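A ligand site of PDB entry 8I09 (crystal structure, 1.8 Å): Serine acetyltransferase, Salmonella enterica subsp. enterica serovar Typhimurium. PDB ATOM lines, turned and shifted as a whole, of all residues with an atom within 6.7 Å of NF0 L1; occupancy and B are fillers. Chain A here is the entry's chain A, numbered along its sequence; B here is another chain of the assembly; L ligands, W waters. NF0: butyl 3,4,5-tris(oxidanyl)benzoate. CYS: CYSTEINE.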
ATOM      1  N   SER A 183      -4.208 -22.288 -20.481  1.00  0.00           N
ATOM      2  CA  SER A 183      -3.613 -21.705 -19.275  1.00  0.00           C
ATOM      3  C   SER A 183      -4.223 -20.306 -19.064  1.00  0.00           C
ATOM      4  O   SER A 183      -4.223 -19.505 -19.991  1.00  0.00           O
ATOM      5  CB  SER A 183      -2.103 -21.626 -19.413  1.00  0.00           C
ATOM      6  OG  SER A 183      -1.555 -22.922 -19.388  1.00  0.00           O
ATOM      7  N   LEU A 185      -4.577 -16.948 -16.283  1.00  0.00           N
ATOM      8  CA  LEU A 185      -4.001 -16.280 -15.111  1.00  0.00           C
ATOM      9  C   LEU A 185      -5.080 -15.583 -14.256  1.00  0.00           C
ATOM     10  O   LEU A 185      -6.263 -15.601 -14.573  1.00  0.00           O
ATOM     11  CB  LEU A 185      -2.846 -15.353 -15.511  1.00  0.00           C
ATOM     12  CG  LEU A 185      -1.490 -16.068 -15.636  1.00  0.00           C
ATOM     13  CD1 LEU A 185      -1.519 -17.229 -16.630  1.00  0.00           C
ATOM     14  CD2 LEU A 185      -0.396 -15.093 -16.018  1.00  0.00           C
ATOM     15  N   MET A 209      -3.347 -19.435 -24.171  1.00  0.00           N
ATOM     16  CA  MET A 209      -2.714 -18.872 -23.006  1.00  0.00           C
ATOM     17  C   MET A 209      -3.356 -17.500 -22.784  1.00  0.00           C
ATOM     18  O   MET A 209      -3.406 -16.693 -23.719  1.00  0.00           O
ATOM     19  CB  MET A 209      -1.225 -18.747 -23.302  1.00  0.00           C
ATOM     20  CG  MET A 209      -0.303 -18.503 -22.117  1.00  0.00           C
ATOM     21  SD  MET A 209       1.384 -18.221 -22.714  1.00  0.00           S
ATOM     22  CE  MET A 209       1.624 -19.678 -23.728  1.00  0.00           C
ATOM     23  N   ILE A 210      -3.872 -17.254 -21.574  1.00  0.00           N
ATOM     24  CA  ILE A 210      -4.530 -15.982 -21.263  1.00  0.00           C
ATOM     25  C   ILE A 210      -3.834 -15.271 -20.107  1.00  0.00           C
ATOM     26  O   ILE A 210      -3.780 -15.769 -18.954  1.00  0.00           O
ATOM     27  CB  ILE A 210      -6.053 -16.147 -20.977  1.00  0.00           C
ATOM     28  CG1 ILE A 210      -6.722 -17.035 -22.048  1.00  0.00           C
ATOM     29  CG2 ILE A 210      -6.737 -14.794 -20.949  1.00  0.00           C
ATOM     30  CD1 ILE A 210      -8.188 -17.329 -21.797  1.00  0.00           C
ATOM     31  N   GLY A 211      -3.295 -14.095 -20.432  1.00  0.00           N
ATOM     32  CA  GLY A 211      -2.569 -13.289 -19.487  1.00  0.00           C
ATOM     33  C   GLY A 211      -3.433 -12.646 -18.407  1.00  0.00           C
ATOM     34  O   GLY A 211      -4.661 -12.592 -18.528  1.00  0.00           O
ATOM     35  N   ALA A 212      -2.748 -12.136 -17.374  1.00  0.00           N
ATOM     36  CA  ALA A 212      -3.361 -11.616 -16.165  1.00  0.00           C
ATOM     37  C   ALA A 212      -4.268 -10.456 -16.492  1.00  0.00           C
ATOM     38  O   ALA A 212      -3.884  -9.565 -17.228  1.00  0.00           O
ATOM     39  CB  ALA A 212      -2.284 -11.180 -15.158  1.00  0.00           C
ATOM     40  N   LYS A 227      -2.471 -16.517 -27.987  1.00  0.00           N
ATOM     41  CA  LYS A 227      -1.981 -15.919 -26.735  1.00  0.00           C
ATOM     42  C   LYS A 227      -2.665 -14.564 -26.523  1.00  0.00           C
ATOM     43  O   LYS A 227      -2.600 -13.687 -27.384  1.00  0.00           O
ATOM     44  CB  LYS A 227      -0.459 -15.751 -26.799  1.00  0.00           C
ATOM     45  CG  LYS A 227       0.164 -15.087 -25.582  1.00  0.00           C
ATOM     46  CD  LYS A 227       1.680 -15.134 -25.667  1.00  0.00           C
ATOM     47  CE  LYS A 227       2.317 -14.246 -24.616  1.00  0.00           C
ATOM     48  NZ  LYS A 227       3.801 -14.379 -24.570  1.00  0.00           N
ATOM     49  N   ILE A 228      -3.347 -14.420 -25.385  1.00  0.00           N
ATOM     50  CA  ILE A 228      -4.038 -13.182 -25.055  1.00  0.00           C
ATOM     51  C   ILE A 228      -3.160 -12.435 -24.051  1.00  0.00           C
ATOM     52  O   ILE A 228      -2.755 -13.000 -23.038  1.00  0.00           O
ATOM     53  CB  ILE A 228      -5.453 -13.429 -24.467  1.00  0.00           C
ATOM     54  CG1 ILE A 228      -6.324 -14.284 -25.419  1.00  0.00           C
ATOM     55  CG2 ILE A 228      -6.151 -12.116 -24.138  1.00  0.00           C
ATOM     56  CD1 ILE A 228      -6.521 -13.717 -26.818  1.00  0.00           C
ATOM     57  N   GLY A 229      -2.875 -11.176 -24.347  1.00  0.00           N
ATOM     58  CA  GLY A 229      -2.010 -10.350 -23.526  1.00  0.00           C
ATOM     59  C   GLY A 229      -2.679  -9.969 -22.215  1.00  0.00           C
ATOM     60  O   GLY A 229      -3.890  -9.809 -22.152  1.00  0.00           O
ATOM     61  N   ALA A 230      -1.862  -9.808 -21.173  1.00  0.00           N
ATOM     62  CA  ALA A 230      -2.307  -9.261 -19.905  1.00  0.00           C
ATOM     63  C   ALA A 230      -3.024  -7.940 -20.139  1.00  0.00           C
ATOM     64  O   ALA A 230      -2.598  -7.153 -20.995  1.00  0.00           O
ATOM     65  CB  ALA A 230      -1.140  -9.067 -18.962  1.00  0.00           C
ATOM     66  N   GLY A 231      -4.134  -7.728 -19.429  1.00  0.00           N
ATOM     67  CA  GLY A 231      -4.872  -6.464 -19.485  1.00  0.00           C
ATOM     68  C   GLY A 231      -5.615  -6.197 -20.778  1.00  0.00           C
ATOM     69  O   GLY A 231      -6.095  -5.083 -20.980  1.00  0.00           O
ATOM     70  N   SER A 232      -5.733  -7.195 -21.662  1.00  0.00           N
ATOM     71  CA  SER A 232      -6.455  -7.025 -22.929  1.00  0.00           C
ATOM     72  C   SER A 232      -7.944  -7.020 -22.718  1.00  0.00           C
ATOM     73  O   SER A 232      -8.447  -7.640 -21.771  1.00  0.00           O
ATOM     74  CB  SER A 232      -6.167  -8.180 -23.878  1.00  0.00           C
ATOM     75  OG  SER A 232      -4.804  -8.215 -24.176  1.00  0.00           O
ATOM     76  N   THR A 243      -1.084 -13.741 -31.390  1.00  0.00           N
ATOM     77  CA  THR A 243      -1.036 -12.992 -30.136  1.00  0.00           C
ATOM     78  C   THR A 243      -1.938 -11.768 -30.297  1.00  0.00           C
ATOM     79  O   THR A 243      -1.694 -10.937 -31.180  1.00  0.00           O
ATOM     80  CB  THR A 243       0.392 -12.528 -29.782  1.00  0.00           C
ATOM     81  OG1 THR A 243       1.264 -13.669 -29.734  1.00  0.00           O
ATOM     82  CG2 THR A 243       0.431 -11.810 -28.429  1.00  0.00           C
ATOM     83  N   ALA A 244      -2.970 -11.680 -29.466  1.00  0.00           N
ATOM     84  CA  ALA A 244      -3.854 -10.512 -29.401  1.00  0.00           C
ATOM     85  C   ALA A 244      -3.605  -9.772 -28.104  1.00  0.00           C
ATOM     86  O   ALA A 244      -3.397 -10.400 -27.060  1.00  0.00           O
ATOM     87  CB  ALA A 244      -5.312 -10.947 -29.474  1.00  0.00           C
ATOM     88  N   ALA A 245      -3.651  -8.438 -28.163  1.00  0.00           N
ATOM     89  CA  ALA A 245      -3.360  -7.613 -27.007  1.00  0.00           C
ATOM     90  C   ALA A 245      -3.852  -6.187 -27.202  1.00  0.00           C
ATOM     91  O   ALA A 245      -4.103  -5.769 -28.322  1.00  0.00           O
ATOM     92  CB  ALA A 245      -1.874  -7.615 -26.715  1.00  0.00           C
ATOM     93  N   GLY A 246      -3.968  -5.468 -26.082  1.00  0.00           N
ATOM     94  CA  GLY A 246      -4.410  -4.069 -26.062  1.00  0.00           C
ATOM     95  C   GLY A 246      -5.845  -3.889 -25.637  1.00  0.00           C
ATOM     96  O   GLY A 246      -6.582  -4.875 -25.443  1.00  0.00           O
ATOM     97  N   VAL A 252      -0.984  -8.569 -32.646  1.00  0.00           N
ATOM     98  CA  VAL A 252       0.341  -7.965 -32.495  1.00  0.00           C
ATOM     99  C   VAL A 252       1.509  -8.894 -32.881  1.00  0.00           C
ATOM    100  O   VAL A 252       2.664  -8.465 -32.851  1.00  0.00           O
ATOM    101  CB  VAL A 252       0.552  -7.410 -31.047  1.00  0.00           C
ATOM    102  CG1 VAL A 252      -0.356  -6.221 -30.791  1.00  0.00           C
ATOM    103  CG2 VAL A 252       0.341  -8.477 -29.981  1.00  0.00           C
ATOM    104  N   GLY B 191       4.683 -10.002 -12.621  1.00  0.00           N
ATOM    105  CA  GLY B 191       4.693 -11.327 -13.238  1.00  0.00           C
ATOM    106  C   GLY B 191       5.671 -11.468 -14.398  1.00  0.00           C
ATOM    107  O   GLY B 191       6.499 -10.596 -14.646  1.00  0.00           O
ATOM    108  N   GLY B 192       5.573 -12.603 -15.100  1.00  0.00           N
ATOM    109  CA  GLY B 192       6.406 -12.908 -16.271  1.00  0.00           C
ATOM    110  C   GLY B 192       5.791 -12.495 -17.606  1.00  0.00           C
ATOM    111  O   GLY B 192       4.682 -11.955 -17.646  1.00  0.00           O
ATOM    112  N   THR B 193       6.538 -12.742 -18.687  1.00  0.00           N
ATOM    113  CA  THR B 193       6.151 -12.436 -20.073  1.00  0.00           C
ATOM    114  C   THR B 193       5.444 -13.615 -20.782  1.00  0.00           C
ATOM    115  O   THR B 193       4.828 -13.446 -21.851  1.00  0.00           O
ATOM    116  CB  THR B 193       7.388 -11.997 -20.909  1.00  0.00           C
ATOM    117  OG1 THR B 193       8.002 -10.865 -20.266  1.00  0.00           O
ATOM    118  CG2 THR B 193       7.014 -11.595 -22.339  1.00  0.00           C
ATOM    119  N   GLY B 194       5.541 -14.801 -20.196  1.00  0.00           N
ATOM    120  CA  GLY B 194       4.807 -15.971 -20.698  1.00  0.00           C
ATOM    121  C   GLY B 194       5.364 -17.219 -20.064  1.00  0.00           C
ATOM    122  O   GLY B 194       5.615 -17.223 -18.854  1.00  0.00           O
ATOM    123  N   LYS B 195       5.566 -18.256 -20.859  1.00  0.00           N
ATOM    124  CA  LYS B 195       6.292 -19.451 -20.380  1.00  0.00           C
ATOM    125  C   LYS B 195       7.802 -19.181 -20.355  1.00  0.00           C
ATOM    126  O   LYS B 195       8.568 -19.668 -21.197  1.00  0.00           O
ATOM    127  CB  LYS B 195       5.893 -20.722 -21.172  1.00  0.00           C
ATOM    128  CG  LYS B 195       6.141 -20.742 -22.678  1.00  0.00           C
ATOM    129  CD  LYS B 195       5.137 -21.631 -23.404  1.00  0.00           C
ATOM    130  CE  LYS B 195       5.089 -23.046 -22.834  1.00  0.00           C
ATOM    131  NZ  LYS B 195       4.382 -23.990 -23.743  1.00  0.00           N
ATOM    132  N   THR B 196       8.221 -18.406 -19.346  1.00  0.00           N
ATOM    133  CA  THR B 196       9.597 -17.930 -19.169  1.00  0.00           C
ATOM    134  C   THR B 196      10.249 -18.638 -17.983  1.00  0.00           C
ATOM    135  O   THR B 196       9.562 -19.337 -17.244  1.00  0.00           O
ATOM    136  CB  THR B 196       9.631 -16.395 -18.942  1.00  0.00           C
ATOM    137  OG1 THR B 196       8.819 -16.047 -17.823  1.00  0.00           O
ATOM    138  CG2 THR B 196       9.124 -15.664 -20.187  1.00  0.00           C
ATOM    139  N   LEU B 217       5.395  -6.760 -16.213  1.00  0.00           N
ATOM    140  CA  LEU B 217       5.736  -8.094 -16.693  1.00  0.00           C
ATOM    141  C   LEU B 217       7.179  -8.160 -17.176  1.00  0.00           C
ATOM    142  O   LEU B 217       7.656  -7.264 -17.873  1.00  0.00           O
ATOM    143  CB  LEU B 217       4.777  -8.513 -17.794  1.00  0.00           C
ATOM    144  CG  LEU B 217       3.283  -8.460 -17.407  1.00  0.00           C
ATOM    145  CD1 LEU B 217       2.401  -8.730 -18.611  1.00  0.00           C
ATOM    146  CD2 LEU B 217       2.931  -9.405 -16.258  1.00  0.00           C
ATOM    147  N   VAL B 233      -0.104  -1.811 -18.573  1.00  0.00           N
ATOM    148  CA  VAL B 233       0.608  -3.030 -18.835  1.00  0.00           C
ATOM    149  C   VAL B 233       2.026  -2.589 -19.209  1.00  0.00           C
ATOM    150  O   VAL B 233       2.273  -2.090 -20.311  1.00  0.00           O
ATOM    151  CB  VAL B 233      -0.079  -3.871 -19.916  1.00  0.00           C
ATOM    152  CG1 VAL B 233       0.711  -5.134 -20.200  1.00  0.00           C
ATOM    153  CG2 VAL B 233      -1.496  -4.235 -19.479  1.00  0.00           C
ATOM    154  N   LEU B 235       5.692  -3.284 -19.998  1.00  0.00           N
ATOM    155  CA  LEU B 235       6.531  -4.305 -20.601  1.00  0.00           C
ATOM    156  C   LEU B 235       7.978  -3.882 -20.820  1.00  0.00           C
ATOM    157  O   LEU B 235       8.797  -4.702 -21.172  1.00  0.00           O
ATOM    158  CB  LEU B 235       5.933  -4.731 -21.937  1.00  0.00           C
ATOM    159  CG  LEU B 235       4.475  -5.205 -21.949  1.00  0.00           C
ATOM    160  CD1 LEU B 235       4.031  -5.534 -23.378  1.00  0.00           C
ATOM    161  CD2 LEU B 235       4.320  -6.412 -21.035  1.00  0.00           C
ATOM    162  N   VAL B 247      -1.902   0.890 -22.066  1.00  0.00           N
ATOM    163  CA  VAL B 247      -1.651  -0.476 -22.540  1.00  0.00           C
ATOM    164  C   VAL B 247      -1.089  -0.432 -23.988  1.00  0.00           C
ATOM    165  O   VAL B 247      -1.855  -0.190 -24.910  1.00  0.00           O
ATOM    166  CB  VAL B 247      -2.926  -1.350 -22.490  1.00  0.00           C
ATOM    167  CG1 VAL B 247      -2.623  -2.764 -22.970  1.00  0.00           C
ATOM    168  CG2 VAL B 247      -3.496  -1.377 -21.070  1.00  0.00           C
ATOM    169  N   PRO B 248       0.211  -0.641 -24.208  1.00  0.00           N
ATOM    170  CA  PRO B 248       1.222  -0.839 -23.183  1.00  0.00           C
ATOM    171  C   PRO B 248       1.614   0.488 -22.576  1.00  0.00           C
ATOM    172  O   PRO B 248       1.245   1.540 -23.098  1.00  0.00           O
ATOM    173  CB  PRO B 248       2.390  -1.426 -23.980  1.00  0.00           C
ATOM    174  CG  PRO B 248       2.270  -0.795 -25.331  1.00  0.00           C
ATOM    175  CD  PRO B 248       0.821  -0.444 -25.543  1.00  0.00           C
HETATM  176  CAL NF0 L   1       1.189  -6.306 -25.631  1.00  0.00           C
HETATM  177  CAK NF0 L   1       0.629  -5.869 -24.318  1.00  0.00           C
HETATM  178  CAJ NF0 L   1       0.558  -7.004 -23.262  1.00  0.00           C
HETATM  179  CAI NF0 L   1       1.073  -8.376 -23.711  1.00  0.00           C
HETATM  180  OAH NF0 L   1       0.996  -9.297 -22.528  1.00  0.00           O
HETATM  181  CAG NF0 L   1       1.672 -10.501 -22.728  1.00  0.00           C
HETATM  182  OAM NF0 L   1       2.474 -10.656 -23.636  1.00  0.00           O
HETATM  183  CAF NF0 L   1       1.481 -11.625 -21.903  1.00  0.00           C
HETATM  184  CAE NF0 L   1       0.589 -12.641 -22.281  1.00  0.00           C
HETATM  185  CAC NF0 L   1       0.444 -13.827 -21.534  1.00  0.00           C
HETATM  186  OAD NF0 L   1      -0.431 -14.824 -21.859  1.00  0.00           O
HETATM  187  CAB NF0 L   1       1.216 -14.008 -20.386  1.00  0.00           C
HETATM  188  OAA NF0 L   1       1.105 -15.142 -19.621  1.00  0.00           O
HETATM  189  CAO NF0 L   1       2.131 -13.028 -20.013  1.00  0.00           C
HETATM  190  OAP NF0 L   1       2.835 -13.301 -18.894  1.00  0.00           O
HETATM  191  CAN NF0 L   1       2.279 -11.848 -20.776  1.00  0.00           C
HETATM  192  N   CYS L   2       3.594 -18.701 -12.142  1.00  0.00           N
HETATM  193  CA  CYS L   2       4.345 -17.998 -13.181  1.00  0.00           C
HETATM  194  C   CYS L   2       5.860 -18.126 -12.989  1.00  0.00           C
HETATM  195  O   CYS L   2       6.355 -18.659 -11.982  1.00  0.00           O
HETATM  196  CB  CYS L   2       3.944 -16.522 -13.234  1.00  0.00           C
HETATM  197  SG  CYS L   2       4.393 -15.561 -11.753  1.00  0.00           S
HETATM  198  OXT CYS L   2       6.631 -17.677 -13.848  1.00  0.00           O
HETATM  199  O   HOH W   1       2.368 -13.077 -15.777  1.00  0.00           O
HETATM  200  O   HOH W   2       0.223 -12.033 -17.575  1.00  0.00           O
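Leu 185 touches NF0 L1 (CD2 to OAA, 3.9 Å). Met 209 touches NF0 L1 (CG to OAD, 3.7 Å). Ile 210 touches NF0 L1 (C to OAD, 3.9 Å). Lys 227 touches NF0 L1. CA of Gly 229 touches OAH of NF0 L1, 3.3 Å away. Ala 245 touches NF0 L1 (CB to CAL, 3.5 Å). Thr 193 of chain B touches NF0 L1. Leu 217 of chain B touches NF0 L1. Val 233 of chain B touches NF0 L1 (CG1 to CAJ, 3.6 Å). Leu 235 of chain B touches NF0 L1 (CD1 to CAK, 3.5 Å). The nearest printed residue that does not touch NF0 L1 is Val 247 of chain B (4.7 Å).
The backbone carbonyl oxygen (O) of Ile 228 lies within hydrogen-bond range of the backbone NH (N) of Gly 211, 2.9 Å away. The backbone carbonyl oxygen (O) of Met 209 sits at hydrogen-bond distance from the backbone NH (N) of Ile 228 (2.8 Å). O of Thr 193 of chain B lies within hydrogen-bond range of NZ of Lys 227, 3.1 Å away. The backbone NH of Ala 244 lies within hydrogen-bond range of the backbone carbonyl oxygen of Lys 227 (2.9 Å). The side-chain hydroxyl (OG) of Ser 232 is in hydrogen-bond range of the backbone carbonyl oxygen (O) of Gly 229 (2.7 Å). The backbone NH (N) of Gly 229 sits at hydrogen-bond distance from the backbone carbonyl oxygen (O) of Ala 244. O of Ile 210 sits at hydrogen-bond distance from N of Leu 185, 3.0 Å away. The backbone NH (N) of Ile 210 lies within hydrogen-bond range of the backbone carbonyl oxygen (O) of Ser 183, at 2.8 Å.
An oxygen (OAP) of NF0 L1 lies within hydrogen-bond range of the backbone carbonyl oxygen (O) of Gly 192 of chain B, 2.6 Å away. The backbone carbonyl oxygen (O) of Ile 228 sits at hydrogen-bond distance from an oxygen (OAD) of NF0 L1, at 3.2 Å. The backbone NH (N) of Ala 230 is in hydrogen-bond range of an oxygen (OAH) of NF0 L1. An oxygen (OAD) of NF0 L1 sits at hydrogen-bond distance from the backbone NH of Gly 211. N of Gly 194 of chain B sits at hydrogen-bond distance from OAP of NF0 L1 (3.4 Å).
Water W1 lies within hydrogen-bond range of OAP of NF0 L1 (3.2 Å) and O of Gly 192 of chain B (3.2 Å). Water W2 bridges N of Ala 212 (3.0 Å) and OAP of NF0 L1 (3.2 Å).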
